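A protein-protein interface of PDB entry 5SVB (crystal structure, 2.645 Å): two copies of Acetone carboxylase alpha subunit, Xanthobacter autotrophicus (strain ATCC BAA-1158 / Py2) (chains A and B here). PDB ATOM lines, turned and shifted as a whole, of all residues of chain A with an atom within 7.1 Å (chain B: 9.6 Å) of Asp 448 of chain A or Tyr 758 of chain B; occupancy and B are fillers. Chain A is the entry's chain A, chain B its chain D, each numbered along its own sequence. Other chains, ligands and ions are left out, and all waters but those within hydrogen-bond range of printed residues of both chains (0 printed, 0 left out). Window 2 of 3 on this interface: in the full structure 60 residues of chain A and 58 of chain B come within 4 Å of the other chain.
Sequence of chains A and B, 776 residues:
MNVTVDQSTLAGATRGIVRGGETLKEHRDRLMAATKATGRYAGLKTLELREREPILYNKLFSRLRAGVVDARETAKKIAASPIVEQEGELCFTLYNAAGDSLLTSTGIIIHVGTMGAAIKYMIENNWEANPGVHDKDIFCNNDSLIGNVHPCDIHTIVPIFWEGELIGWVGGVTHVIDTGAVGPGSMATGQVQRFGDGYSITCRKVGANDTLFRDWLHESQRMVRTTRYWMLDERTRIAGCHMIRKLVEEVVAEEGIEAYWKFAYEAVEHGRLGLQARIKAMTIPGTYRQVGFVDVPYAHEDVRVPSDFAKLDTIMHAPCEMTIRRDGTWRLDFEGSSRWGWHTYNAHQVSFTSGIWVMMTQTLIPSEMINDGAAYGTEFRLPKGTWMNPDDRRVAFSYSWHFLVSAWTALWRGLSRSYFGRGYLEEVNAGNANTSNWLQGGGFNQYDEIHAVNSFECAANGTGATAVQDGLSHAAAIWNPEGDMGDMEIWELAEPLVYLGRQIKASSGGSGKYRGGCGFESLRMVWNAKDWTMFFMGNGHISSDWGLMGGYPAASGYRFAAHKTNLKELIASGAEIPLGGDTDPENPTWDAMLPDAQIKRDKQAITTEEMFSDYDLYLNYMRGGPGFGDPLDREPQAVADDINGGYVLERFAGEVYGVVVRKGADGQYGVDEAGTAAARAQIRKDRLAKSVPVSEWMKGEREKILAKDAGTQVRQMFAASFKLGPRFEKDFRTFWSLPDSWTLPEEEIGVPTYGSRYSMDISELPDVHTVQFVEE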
ATOM      1  N   PHE A 444     -11.256 -32.228  -0.697  1.00  0.00           N
ATOM      2  CA  PHE A 444     -12.200 -33.291  -1.009  1.00  0.00           C
ATOM      3  C   PHE A 444     -11.727 -34.047  -2.242  1.00  0.00           C
ATOM      4  O   PHE A 444     -11.175 -33.455  -3.173  1.00  0.00           O
ATOM      5  CB  PHE A 444     -13.605 -32.724  -1.221  1.00  0.00           C
ATOM      6  CG  PHE A 444     -14.226 -32.182   0.033  1.00  0.00           C
ATOM      7  CD1 PHE A 444     -13.843 -30.953   0.536  1.00  0.00           C
ATOM      8  CD2 PHE A 444     -15.187 -32.907   0.716  1.00  0.00           C
ATOM      9  CE1 PHE A 444     -14.407 -30.454   1.690  1.00  0.00           C
ATOM     10  CE2 PHE A 444     -15.754 -32.412   1.872  1.00  0.00           C
ATOM     11  CZ  PHE A 444     -15.364 -31.186   2.360  1.00  0.00           C
ATOM     12  N   ASN A 445     -11.951 -35.355  -2.239  1.00  0.00           N
ATOM     13  CA  ASN A 445     -11.319 -36.263  -3.181  1.00  0.00           C
ATOM     14  C   ASN A 445     -12.281 -36.630  -4.311  1.00  0.00           C
ATOM     15  O   ASN A 445     -13.373 -36.073  -4.438  1.00  0.00           O
ATOM     16  CB  ASN A 445     -10.824 -37.503  -2.434  1.00  0.00           C
ATOM     17  CG  ASN A 445     -11.941 -38.238  -1.720  1.00  0.00           C
ATOM     18  OD1 ASN A 445     -13.106 -38.148  -2.104  1.00  0.00           O
ATOM     19  ND2 ASN A 445     -11.590 -38.968  -0.669  1.00  0.00           N
ATOM     20  N   GLN A 446     -11.867 -37.589  -5.144  1.00  0.00           N
ATOM     21  CA  GLN A 446     -12.680 -38.033  -6.269  1.00  0.00           C
ATOM     22  C   GLN A 446     -13.943 -38.758  -5.834  1.00  0.00           C
ATOM     23  O   GLN A 446     -14.768 -39.091  -6.690  1.00  0.00           O
ATOM     24  CB  GLN A 446     -11.865 -38.945  -7.186  1.00  0.00           C
ATOM     25  CG  GLN A 446     -11.374 -40.237  -6.542  1.00  0.00           C
ATOM     26  CD  GLN A 446     -10.035 -40.078  -5.859  1.00  0.00           C
ATOM     27  OE1 GLN A 446      -9.827 -39.146  -5.087  1.00  0.00           O
ATOM     28  NE2 GLN A 446      -9.114 -40.984  -6.149  1.00  0.00           N
ATOM     29  N   TYR A 447     -14.104 -39.026  -4.541  1.00  0.00           N
ATOM     30  CA  TYR A 447     -15.329 -39.595  -4.005  1.00  0.00           C
ATOM     31  C   TYR A 447     -16.223 -38.537  -3.378  1.00  0.00           C
ATOM     32  O   TYR A 447     -17.256 -38.875  -2.796  1.00  0.00           O
ATOM     33  CB  TYR A 447     -14.995 -40.678  -2.978  1.00  0.00           C
ATOM     34  CG  TYR A 447     -13.954 -41.662  -3.459  1.00  0.00           C
ATOM     35  CD1 TYR A 447     -14.255 -42.597  -4.437  1.00  0.00           C
ATOM     36  CD2 TYR A 447     -12.667 -41.653  -2.937  1.00  0.00           C
ATOM     37  CE1 TYR A 447     -13.309 -43.495  -4.882  1.00  0.00           C
ATOM     38  CE2 TYR A 447     -11.714 -42.548  -3.375  1.00  0.00           C
ATOM     39  CZ  TYR A 447     -12.041 -43.468  -4.347  1.00  0.00           C
ATOM     40  OH  TYR A 447     -11.096 -44.362  -4.790  1.00  0.00           O
ATOM     41  N   ASP A 448     -15.851 -37.263  -3.495  1.00  0.00           N
ATOM     42  CA  ASP A 448     -16.575 -36.171  -2.851  1.00  0.00           C
ATOM     43  C   ASP A 448     -16.604 -36.348  -1.340  1.00  0.00           C
ATOM     44  O   ASP A 448     -17.568 -35.966  -0.675  1.00  0.00           O
ATOM     45  CB  ASP A 448     -17.994 -36.043  -3.409  1.00  0.00           C
ATOM     46  CG  ASP A 448     -18.008 -35.631  -4.866  1.00  0.00           C
ATOM     47  OD1 ASP A 448     -17.103 -34.876  -5.274  1.00  0.00           O
ATOM     48  OD2 ASP A 448     -18.919 -36.060  -5.603  1.00  0.00           O
ATOM     49  N   GLU A 449     -15.542 -36.928  -0.794  1.00  0.00           N
ATOM     50  CA  GLU A 449     -15.405 -37.147   0.636  1.00  0.00           C
ATOM     51  C   GLU A 449     -14.107 -36.518   1.122  1.00  0.00           C
ATOM     52  O   GLU A 449     -13.208 -36.208   0.337  1.00  0.00           O
ATOM     53  CB  GLU A 449     -15.434 -38.643   0.969  1.00  0.00           C
ATOM     54  CG  GLU A 449     -16.563 -39.387   0.274  1.00  0.00           C
ATOM     55  CD  GLU A 449     -16.785 -40.777   0.829  1.00  0.00           C
ATOM     56  OE1 GLU A 449     -15.799 -41.530   0.962  1.00  0.00           O
ATOM     57  OE2 GLU A 449     -17.948 -41.114   1.136  1.00  0.00           O
ATOM     58  N   ILE A 450     -14.023 -36.325   2.439  1.00  0.00           N
ATOM     59  CA  ILE A 450     -12.856 -35.677   3.020  1.00  0.00           C
ATOM     60  C   ILE A 450     -11.611 -36.509   2.748  1.00  0.00           C
ATOM     61  O   ILE A 450     -11.619 -37.742   2.865  1.00  0.00           O
ATOM     62  CB  ILE A 450     -13.057 -35.462   4.528  1.00  0.00           C
ATOM     63  CG1 ILE A 450     -14.315 -34.630   4.783  1.00  0.00           C
ATOM     64  CG2 ILE A 450     -11.844 -34.769   5.135  1.00  0.00           C
ATOM     65  CD1 ILE A 450     -15.116 -35.112   5.963  1.00  0.00           C
ATOM     66  N   ASN A 528      -9.881 -34.581 -10.256  1.00  0.00           N
ATOM     67  CA  ASN A 528     -11.132 -34.803  -9.529  1.00  0.00           C
ATOM     68  C   ASN A 528     -11.014 -34.389  -8.062  1.00  0.00           C
ATOM     69  O   ASN A 528     -11.592 -35.021  -7.181  1.00  0.00           O
ATOM     70  CB  ASN A 528     -11.593 -36.258  -9.644  1.00  0.00           C
ATOM     71  CG  ASN A 528     -12.045 -36.613 -11.045  1.00  0.00           C
ATOM     72  OD1 ASN A 528     -12.617 -35.785 -11.752  1.00  0.00           O
ATOM     73  ND2 ASN A 528     -11.790 -37.849 -11.454  1.00  0.00           N
ATOM     74  N   ALA A 529     -10.273 -33.319  -7.804  1.00  0.00           N
ATOM     75  CA  ALA A 529     -10.180 -32.736  -6.475  1.00  0.00           C
ATOM     76  C   ALA A 529     -11.112 -31.535  -6.361  1.00  0.00           C
ATOM     77  O   ALA A 529     -11.468 -30.896  -7.354  1.00  0.00           O
ATOM     78  CB  ALA A 529      -8.744 -32.313  -6.164  1.00  0.00           C
ATOM     79  N   LYS A 530     -11.511 -31.238  -5.127  1.00  0.00           N
ATOM     80  CA  LYS A 530     -12.342 -30.080  -4.838  1.00  0.00           C
ATOM     81  C   LYS A 530     -11.868 -29.444  -3.542  1.00  0.00           C
ATOM     82  O   LYS A 530     -11.501 -30.148  -2.597  1.00  0.00           O
ATOM     83  CB  LYS A 530     -13.823 -30.462  -4.729  1.00  0.00           C
ATOM     84  CG  LYS A 530     -14.365 -31.201  -5.942  1.00  0.00           C
ATOM     85  CD  LYS A 530     -14.462 -32.692  -5.682  1.00  0.00           C
ATOM     86  CE  LYS A 530     -14.688 -33.465  -6.966  1.00  0.00           C
ATOM     87  NZ  LYS A 530     -14.989 -34.897  -6.698  1.00  0.00           N
ATOM     88  N   ASP A 531     -11.878 -28.113  -3.504  1.00  0.00           N
ATOM     89  CA  ASP A 531     -11.387 -27.363  -2.348  1.00  0.00           C
ATOM     90  C   ASP A 531     -10.018 -27.886  -1.923  1.00  0.00           C
ATOM     91  O   ASP A 531      -9.757 -28.154  -0.750  1.00  0.00           O
ATOM     92  CB  ASP A 531     -12.387 -27.429  -1.193  1.00  0.00           C
ATOM     93  CG  ASP A 531     -13.701 -26.745  -1.518  1.00  0.00           C
ATOM     94  OD1 ASP A 531     -13.880 -26.319  -2.678  1.00  0.00           O
ATOM     95  OD2 ASP A 531     -14.558 -26.639  -0.617  1.00  0.00           O
ATOM     96  N   ARG B 339     -23.552 -16.919   4.291  1.00  0.00           N
ATOM     97  CA  ARG B 339     -22.940 -18.174   4.688  1.00  0.00           C
ATOM     98  C   ARG B 339     -21.849 -17.929   5.725  1.00  0.00           C
ATOM     99  O   ARG B 339     -21.327 -16.820   5.871  1.00  0.00           O
ATOM    100  CB  ARG B 339     -22.354 -18.885   3.466  1.00  0.00           C
ATOM    101  CG  ARG B 339     -21.860 -20.295   3.737  1.00  0.00           C
ATOM    102  CD  ARG B 339     -21.449 -21.017   2.467  1.00  0.00           C
ATOM    103  NE  ARG B 339     -20.189 -20.511   1.920  1.00  0.00           N
ATOM    104  CZ  ARG B 339     -20.072 -19.733   0.848  1.00  0.00           C
ATOM    105  NH1 ARG B 339     -21.139 -19.345   0.163  1.00  0.00           N
ATOM    106  NH2 ARG B 339     -18.869 -19.342   0.450  1.00  0.00           N
ATOM    107  N   TRP B 340     -21.517 -18.982   6.464  1.00  0.00           N
ATOM    108  CA  TRP B 340     -20.354 -18.932   7.329  1.00  0.00           C
ATOM    109  C   TRP B 340     -19.092 -18.789   6.485  1.00  0.00           C
ATOM    110  O   TRP B 340     -19.062 -19.133   5.301  1.00  0.00           O
ATOM    111  CB  TRP B 340     -20.275 -20.186   8.197  1.00  0.00           C
ATOM    112  CG  TRP B 340     -20.062 -21.448   7.419  1.00  0.00           C
ATOM    113  CD1 TRP B 340     -21.019 -22.302   6.965  1.00  0.00           C
ATOM    114  CD2 TRP B 340     -18.806 -21.998   7.009  1.00  0.00           C
ATOM    115  NE1 TRP B 340     -20.441 -23.349   6.297  1.00  0.00           N
ATOM    116  CE2 TRP B 340     -19.080 -23.186   6.308  1.00  0.00           C
ATOM    117  CE3 TRP B 340     -17.475 -21.601   7.164  1.00  0.00           C
ATOM    118  CZ2 TRP B 340     -18.076 -23.982   5.766  1.00  0.00           C
ATOM    119  CZ3 TRP B 340     -16.480 -22.389   6.624  1.00  0.00           C
ATOM    120  CH2 TRP B 340     -16.784 -23.565   5.935  1.00  0.00           C
ATOM    121  N   TRP B 342     -14.462 -18.341   6.440  1.00  0.00           N
ATOM    122  CA  TRP B 342     -13.174 -18.683   7.021  1.00  0.00           C
ATOM    123  C   TRP B 342     -12.711 -17.569   7.948  1.00  0.00           C
ATOM    124  O   TRP B 342     -11.987 -16.660   7.533  1.00  0.00           O
ATOM    125  CB  TRP B 342     -12.154 -18.942   5.915  1.00  0.00           C
ATOM    126  CG  TRP B 342     -12.605 -20.006   4.972  1.00  0.00           C
ATOM    127  CD1 TRP B 342     -13.045 -19.837   3.694  1.00  0.00           C
ATOM    128  CD2 TRP B 342     -12.684 -21.409   5.243  1.00  0.00           C
ATOM    129  NE1 TRP B 342     -13.384 -21.049   3.146  1.00  0.00           N
ATOM    130  CE2 TRP B 342     -13.172 -22.031   4.077  1.00  0.00           C
ATOM    131  CE3 TRP B 342     -12.385 -22.198   6.354  1.00  0.00           C
ATOM    132  CZ2 TRP B 342     -13.367 -23.406   3.993  1.00  0.00           C
ATOM    133  CZ3 TRP B 342     -12.579 -23.561   6.269  1.00  0.00           C
ATOM    134  CH2 TRP B 342     -13.064 -24.152   5.097  1.00  0.00           C
ATOM    135  N   PRO B 390     -24.116 -22.815  11.276  1.00  0.00           N
ATOM    136  CA  PRO B 390     -23.298 -23.332  10.165  1.00  0.00           C
ATOM    137  C   PRO B 390     -23.504 -24.809   9.883  1.00  0.00           C
ATOM    138  O   PRO B 390     -23.543 -25.208   8.714  1.00  0.00           O
ATOM    139  CB  PRO B 390     -21.865 -23.038  10.629  1.00  0.00           C
ATOM    140  CG  PRO B 390     -21.994 -22.016  11.705  1.00  0.00           C
ATOM    141  CD  PRO B 390     -23.286 -22.299  12.375  1.00  0.00           C
ATOM    142  N   ASP B 391     -23.618 -25.636  10.918  1.00  0.00           N
ATOM    143  CA  ASP B 391     -23.737 -27.083  10.744  1.00  0.00           C
ATOM    144  C   ASP B 391     -22.545 -27.643   9.969  1.00  0.00           C
ATOM    145  O   ASP B 391     -22.690 -28.520   9.115  1.00  0.00           O
ATOM    146  CB  ASP B 391     -25.052 -27.449  10.050  1.00  0.00           C
ATOM    147  CG  ASP B 391     -25.386 -28.926  10.173  1.00  0.00           C
ATOM    148  OD1 ASP B 391     -25.122 -29.511  11.244  1.00  0.00           O
ATOM    149  OD2 ASP B 391     -25.912 -29.503   9.199  1.00  0.00           O
ATOM    150  N   ASP B 392     -21.354 -27.124  10.265  1.00  0.00           N
ATOM    151  CA  ASP B 392     -20.116 -27.588   9.651  1.00  0.00           C
ATOM    152  C   ASP B 392     -19.032 -27.579  10.714  1.00  0.00           C
ATOM    153  O   ASP B 392     -18.865 -26.583  11.420  1.00  0.00           O
ATOM    154  CB  ASP B 392     -19.717 -26.704   8.465  1.00  0.00           C
ATOM    155  CG  ASP B 392     -18.594 -27.301   7.641  1.00  0.00           C
ATOM    156  OD1 ASP B 392     -17.434 -27.278   8.101  1.00  0.00           O
ATOM    157  OD2 ASP B 392     -18.868 -27.786   6.525  1.00  0.00           O
ATOM    158  N   ARG B 393     -18.295 -28.685  10.829  1.00  0.00           N
ATOM    159  CA  ARG B 393     -17.383 -28.864  11.956  1.00  0.00           C
ATOM    160  C   ARG B 393     -16.087 -28.077  11.805  1.00  0.00           C
ATOM    161  O   ARG B 393     -15.363 -27.922  12.794  1.00  0.00           O
ATOM    162  CB  ARG B 393     -17.049 -30.343  12.169  1.00  0.00           C
ATOM    163  CG  ARG B 393     -18.024 -31.329  11.532  1.00  0.00           C
ATOM    164  CD  ARG B 393     -18.069 -32.667  12.255  1.00  0.00           C
ATOM    165  NE  ARG B 393     -17.334 -33.715  11.551  1.00  0.00           N
ATOM    166  CZ  ARG B 393     -16.144 -34.189  11.906  1.00  0.00           C
ATOM    167  NH1 ARG B 393     -15.506 -33.724  12.974  1.00  0.00           N
ATOM    168  NH2 ARG B 393     -15.582 -35.147  11.184  1.00  0.00           N
ATOM    169  N   ARG B 394     -15.774 -27.585  10.607  1.00  0.00           N
ATOM    170  CA  ARG B 394     -14.585 -26.764  10.421  1.00  0.00           C
ATOM    171  C   ARG B 394     -14.757 -25.350  10.958  1.00  0.00           C
ATOM    172  O   ARG B 394     -13.759 -24.647  11.144  1.00  0.00           O
ATOM    173  CB  ARG B 394     -14.224 -26.689   8.937  1.00  0.00           C
ATOM    174  CG  ARG B 394     -13.726 -27.989   8.336  1.00  0.00           C
ATOM    175  CD  ARG B 394     -13.674 -27.899   6.820  1.00  0.00           C
ATOM    176  NE  ARG B 394     -15.005 -27.753   6.239  1.00  0.00           N
ATOM    177  CZ  ARG B 394     -15.246 -27.630   4.938  1.00  0.00           C
ATOM    178  NH1 ARG B 394     -14.247 -27.630   4.065  1.00  0.00           N
ATOM    179  NH2 ARG B 394     -16.493 -27.506   4.509  1.00  0.00           N
ATOM    180  N   VAL B 395     -15.992 -24.922  11.214  1.00  0.00           N
ATOM    181  CA  VAL B 395     -16.263 -23.520  11.504  1.00  0.00           C
ATOM    182  C   VAL B 395     -15.628 -23.118  12.826  1.00  0.00           C
ATOM    183  O   VAL B 395     -15.683 -23.857  13.818  1.00  0.00           O
ATOM    184  CB  VAL B 395     -17.778 -23.267  11.521  1.00  0.00           C
ATOM    185  CG1 VAL B 395     -18.082 -21.839  11.949  1.00  0.00           C
ATOM    186  CG2 VAL B 395     -18.355 -23.536  10.155  1.00  0.00           C
ATOM    187  N   LYS B 723     -28.101 -18.679  -2.192  1.00  0.00           N
ATOM    188  CA  LYS B 723     -28.075 -20.136  -2.144  1.00  0.00           C
ATOM    189  C   LYS B 723     -28.661 -20.664  -0.841  1.00  0.00           C
ATOM    190  O   LYS B 723     -29.350 -21.691  -0.833  1.00  0.00           O
ATOM    191  CB  LYS B 723     -26.645 -20.639  -2.332  1.00  0.00           C
ATOM    192  CG  LYS B 723     -26.158 -20.556  -3.765  1.00  0.00           C
ATOM    193  CD  LYS B 723     -24.772 -21.151  -3.928  1.00  0.00           C
ATOM    194  CE  LYS B 723     -23.697 -20.219  -3.400  1.00  0.00           C
ATOM    195  NZ  LYS B 723     -22.330 -20.763  -3.645  1.00  0.00           N
ATOM    196  N   GLU B 747     -19.335 -18.664  -7.872  1.00  0.00           N
ATOM    197  CA  GLU B 747     -18.150 -19.269  -8.461  1.00  0.00           C
ATOM    198  C   GLU B 747     -17.569 -18.436  -9.595  1.00  0.00           C
ATOM    199  O   GLU B 747     -16.485 -18.765 -10.088  1.00  0.00           O
ATOM    200  CB  GLU B 747     -18.487 -20.677  -8.968  1.00  0.00           C
ATOM    201  CG  GLU B 747     -19.121 -21.608  -7.921  1.00  0.00           C
ATOM    202  CD  GLU B 747     -20.616 -21.376  -7.724  1.00  0.00           C
ATOM    203  OE1 GLU B 747     -21.211 -20.588  -8.489  1.00  0.00           O
ATOM    204  OE2 GLU B 747     -21.199 -21.980  -6.798  1.00  0.00           O
ATOM    205  N   THR B 753     -13.804 -19.707  -3.144  1.00  0.00           N
ATOM    206  CA  THR B 753     -15.120 -20.168  -2.723  1.00  0.00           C
ATOM    207  C   THR B 753     -15.029 -21.513  -2.015  1.00  0.00           C
ATOM    208  O   THR B 753     -15.986 -22.288  -2.018  1.00  0.00           O
ATOM    209  CB  THR B 753     -16.079 -20.257  -3.911  1.00  0.00           C
ATOM    210  OG1 THR B 753     -15.632 -21.264  -4.823  1.00  0.00           O
ATOM    211  CG2 THR B 753     -16.154 -18.925  -4.633  1.00  0.00           C
ATOM    212  N   TYR B 754     -13.890 -21.802  -1.396  1.00  0.00           N
ATOM    213  CA  TYR B 754     -13.748 -23.040  -0.644  1.00  0.00           C
ATOM    214  C   TYR B 754     -14.783 -23.096   0.472  1.00  0.00           C
ATOM    215  O   TYR B 754     -14.912 -22.159   1.264  1.00  0.00           O
ATOM    216  CB  TYR B 754     -12.337 -23.154  -0.065  1.00  0.00           C
ATOM    217  CG  TYR B 754     -11.287 -23.603  -1.059  1.00  0.00           C
ATOM    218  CD1 TYR B 754     -11.467 -23.419  -2.422  1.00  0.00           C
ATOM    219  CD2 TYR B 754     -10.123 -24.222  -0.635  1.00  0.00           C
ATOM    220  CE1 TYR B 754     -10.512 -23.835  -3.329  1.00  0.00           C
ATOM    221  CE2 TYR B 754      -9.164 -24.640  -1.535  1.00  0.00           C
ATOM    222  CZ  TYR B 754      -9.365 -24.444  -2.881  1.00  0.00           C
ATOM    223  OH  TYR B 754      -8.415 -24.857  -3.785  1.00  0.00           O
ATOM    224  N   GLY B 755     -15.526 -24.197   0.526  1.00  0.00           N
ATOM    225  CA  GLY B 755     -16.542 -24.398   1.534  1.00  0.00           C
ATOM    226  C   GLY B 755     -17.944 -24.017   1.116  1.00  0.00           C
ATOM    227  O   GLY B 755     -18.858 -24.088   1.946  1.00  0.00           O
ATOM    228  N   SER B 756     -18.150 -23.627  -0.141  1.00  0.00           N
ATOM    229  CA  SER B 756     -19.464 -23.197  -0.597  1.00  0.00           C
ATOM    230  C   SER B 756     -20.319 -24.345  -1.113  1.00  0.00           C
ATOM    231  O   SER B 756     -21.551 -24.262  -1.052  1.00  0.00           O
ATOM    232  CB  SER B 756     -19.318 -22.144  -1.699  1.00  0.00           C
ATOM    233  OG  SER B 756     -18.818 -22.718  -2.891  1.00  0.00           O
ATOM    234  N   ARG B 757     -19.698 -25.412  -1.618  1.00  0.00           N
ATOM    235  CA  ARG B 757     -20.422 -26.550  -2.166  1.00  0.00           C
ATOM    236  C   ARG B 757     -20.069 -27.878  -1.514  1.00  0.00           C
ATOM    237  O   ARG B 757     -20.821 -28.842  -1.685  1.00  0.00           O
ATOM    238  CB  ARG B 757     -20.172 -26.669  -3.677  1.00  0.00           C
ATOM    239  CG  ARG B 757     -20.894 -25.619  -4.513  1.00  0.00           C
ATOM    240  CD  ARG B 757     -20.443 -25.652  -5.965  1.00  0.00           C
ATOM    241  NE  ARG B 757     -20.334 -27.017  -6.473  1.00  0.00           N
ATOM    242  CZ  ARG B 757     -21.369 -27.774  -6.817  1.00  0.00           C
ATOM    243  NH1 ARG B 757     -22.608 -27.308  -6.705  1.00  0.00           N
ATOM    244  NH2 ARG B 757     -21.168 -29.006  -7.267  1.00  0.00           N
ATOM    245  N   TYR B 758     -18.961 -27.959  -0.785  1.00  0.00           N
ATOM    246  CA  TYR B 758     -18.561 -29.169  -0.081  1.00  0.00           C
ATOM    247  C   TYR B 758     -18.471 -28.855   1.403  1.00  0.00           C
ATOM    248  O   TYR B 758     -17.877 -27.845   1.791  1.00  0.00           O
ATOM    249  CB  TYR B 758     -17.225 -29.695  -0.615  1.00  0.00           C
ATOM    250  CG  TYR B 758     -17.322 -30.211  -2.033  1.00  0.00           C
ATOM    251  CD1 TYR B 758     -17.147 -29.362  -3.115  1.00  0.00           C
ATOM    252  CD2 TYR B 758     -17.604 -31.543  -2.284  1.00  0.00           C
ATOM    253  CE1 TYR B 758     -17.244 -29.829  -4.409  1.00  0.00           C
ATOM    254  CE2 TYR B 758     -17.703 -32.019  -3.573  1.00  0.00           C
ATOM    255  CZ  TYR B 758     -17.523 -31.160  -4.631  1.00  0.00           C
ATOM    256  OH  TYR B 758     -17.621 -31.639  -5.917  1.00  0.00           O
ATOM    257  N   SER B 759     -19.067 -29.713   2.226  1.00  0.00           N
ATOM    258  CA  SER B 759     -19.274 -29.417   3.633  1.00  0.00           C
ATOM    259  C   SER B 759     -18.826 -30.582   4.503  1.00  0.00           C
ATOM    260  O   SER B 759     -18.653 -31.710   4.037  1.00  0.00           O
ATOM    261  CB  SER B 759     -20.747 -29.101   3.918  1.00  0.00           C
ATOM    262  OG  SER B 759     -21.161 -27.937   3.222  1.00  0.00           O
ATOM    263  N   MET B 760     -18.638 -30.278   5.782  1.00  0.00           N
ATOM    264  CA  MET B 760     -18.348 -31.282   6.797  1.00  0.00           C
ATOM    265  C   MET B 760     -19.463 -31.259   7.838  1.00  0.00           C
ATOM    266  O   MET B 760     -19.305 -30.697   8.919  1.00  0.00           O
ATOM    267  CB  MET B 760     -16.988 -31.018   7.450  1.00  0.00           C
ATOM    268  CG  MET B 760     -15.905 -31.988   7.031  1.00  0.00           C
ATOM    269  SD  MET B 760     -14.188 -31.674   7.909  1.00  0.00           S
ATOM    270  CE  MET B 760     -14.567 -32.502   9.631  1.00  0.00           C
ATOM    271  N   ASP B 761     -20.598 -31.863   7.502  1.00  0.00           N
ATOM    272  CA  ASP B 761     -21.750 -31.830   8.388  1.00  0.00           C
ATOM    273  C   ASP B 761     -21.416 -32.472   9.732  1.00  0.00           C
ATOM    274  O   ASP B 761     -20.464 -33.243   9.868  1.00  0.00           O
ATOM    275  CB  ASP B 761     -22.935 -32.555   7.754  1.00  0.00           C
ATOM    276  CG  ASP B 761     -23.342 -31.954   6.423  1.00  0.00           C
ATOM    277  OD1 ASP B 761     -22.777 -32.363   5.387  1.00  0.00           O
ATOM    278  OD2 ASP B 761     -24.228 -31.075   6.414  1.00  0.00           O
ATOM    279  N   GLU B 764     -22.215 -36.412   9.953  1.00  0.00           N
ATOM    280  CA  GLU B 764     -21.187 -37.412   9.692  1.00  0.00           C
ATOM    281  C   GLU B 764     -20.770 -38.117  10.977  1.00  0.00           C
ATOM    282  O   GLU B 764     -20.543 -39.333  10.981  1.00  0.00           O
ATOM    283  CB  GLU B 764     -19.976 -36.757   9.025  1.00  0.00           C
ATOM    284  CG  GLU B 764     -20.232 -36.282   7.602  1.00  0.00           C
ATOM    285  CD  GLU B 764     -19.115 -35.404   7.070  1.00  0.00           C
ATOM    286  OE1 GLU B 764     -18.047 -35.342   7.715  1.00  0.00           O
ATOM    287  OE2 GLU B 764     -19.306 -34.773   6.009  1.00  0.00           O
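Phe 444 of chain A touches Arg 394 of chain B (CE1 to NH1, 3.7 Å).
Phe 444 of chain A touches Tyr 758 of chain B.
Phe 444 of chain A touches Ser 759 of chain B.
CD1 of Ile 450 of chain A touches CG of Met 760 of chain B, at 3.4 Å.
Ile 450 of chain A touches Glu 764 of chain B (CD1 to OE1, 3.4 Å).
OH of Tyr 758 of chain B touches CG of Lys 530 of chain A, 3.3 Å away.
Asp 531 of chain A touches Tyr 754 of chain B (C to CE2, 3.4 Å).
The backbone NH of Phe 444 of chain A lies within hydrogen-bond range of the backbone carbonyl oxygen of Lys 530 of chain A, 2.8 Å away.
NZ of Lys 530 of chain A sits at hydrogen-bond distance from O of Asn 445 of chain A.
The side-chain carboxylate of Asp 448 of chain A is in salt-bridge range of the side-chain amino group of Lys 530 of chain A (2.5 Å).
O of Asn 528 of chain A sits at hydrogen-bond distance from NZ of Lys 530 of chain A (3.4 Å).
NE of Arg 394 of chain B lies within salt-bridge range of OD1 of Asp 392 of chain B.
The backbone NH of Arg 393 of chain B lies within hydrogen-bond range of the backbone carbonyl oxygen of Met 760 of chain B (3.0 Å).
OD1 of Asp 448 of chain A lies within hydrogen-bond range of OH of Tyr 758 of chain B, at 3.3 Å.
OD2 of Asp 531 of chain A lies within hydrogen-bond range of N of Gly 755 of chain B, 2.9 Å away.
Of the 21 printed residues of chain B, 7 touch a printed residue of chain A.
Among the printed residues, 9 pairs touch across the chains.
Among the printed residues, no Asp or Glu carboxylate lies within 4 Å of a Lys or Arg side-chain nitrogen of the other chain.
No residue of chain B comes within 4 Å of Asn 445 of chain A.
Asn 528 of chain A touches none of the printed residues of chain B.
Of the printed residues of chain B, Asp 531 of chain A touches Tyr 754 (3.4 Å) and Gly 755 (2.9 Å).
Printed residues of chain A within 4 Å of Arg 394 of chain B: Phe 444 (3.7 Å).
Ser 756 of chain B touches none of the printed residues of chain A.
Of chain A, only Phe 444, Asp 448 and Lys 530 come within 4 Å of Tyr 758 of chain B.
Printed residues of chain A within 4 Å of Ser 759 of chain B: Phe 444 (3.7 Å).
The nearest residue of chain A that does not touch Tyr 758 of chain B is Asp 531 of chain A (4.1 Å).
No position is printed for both chains.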
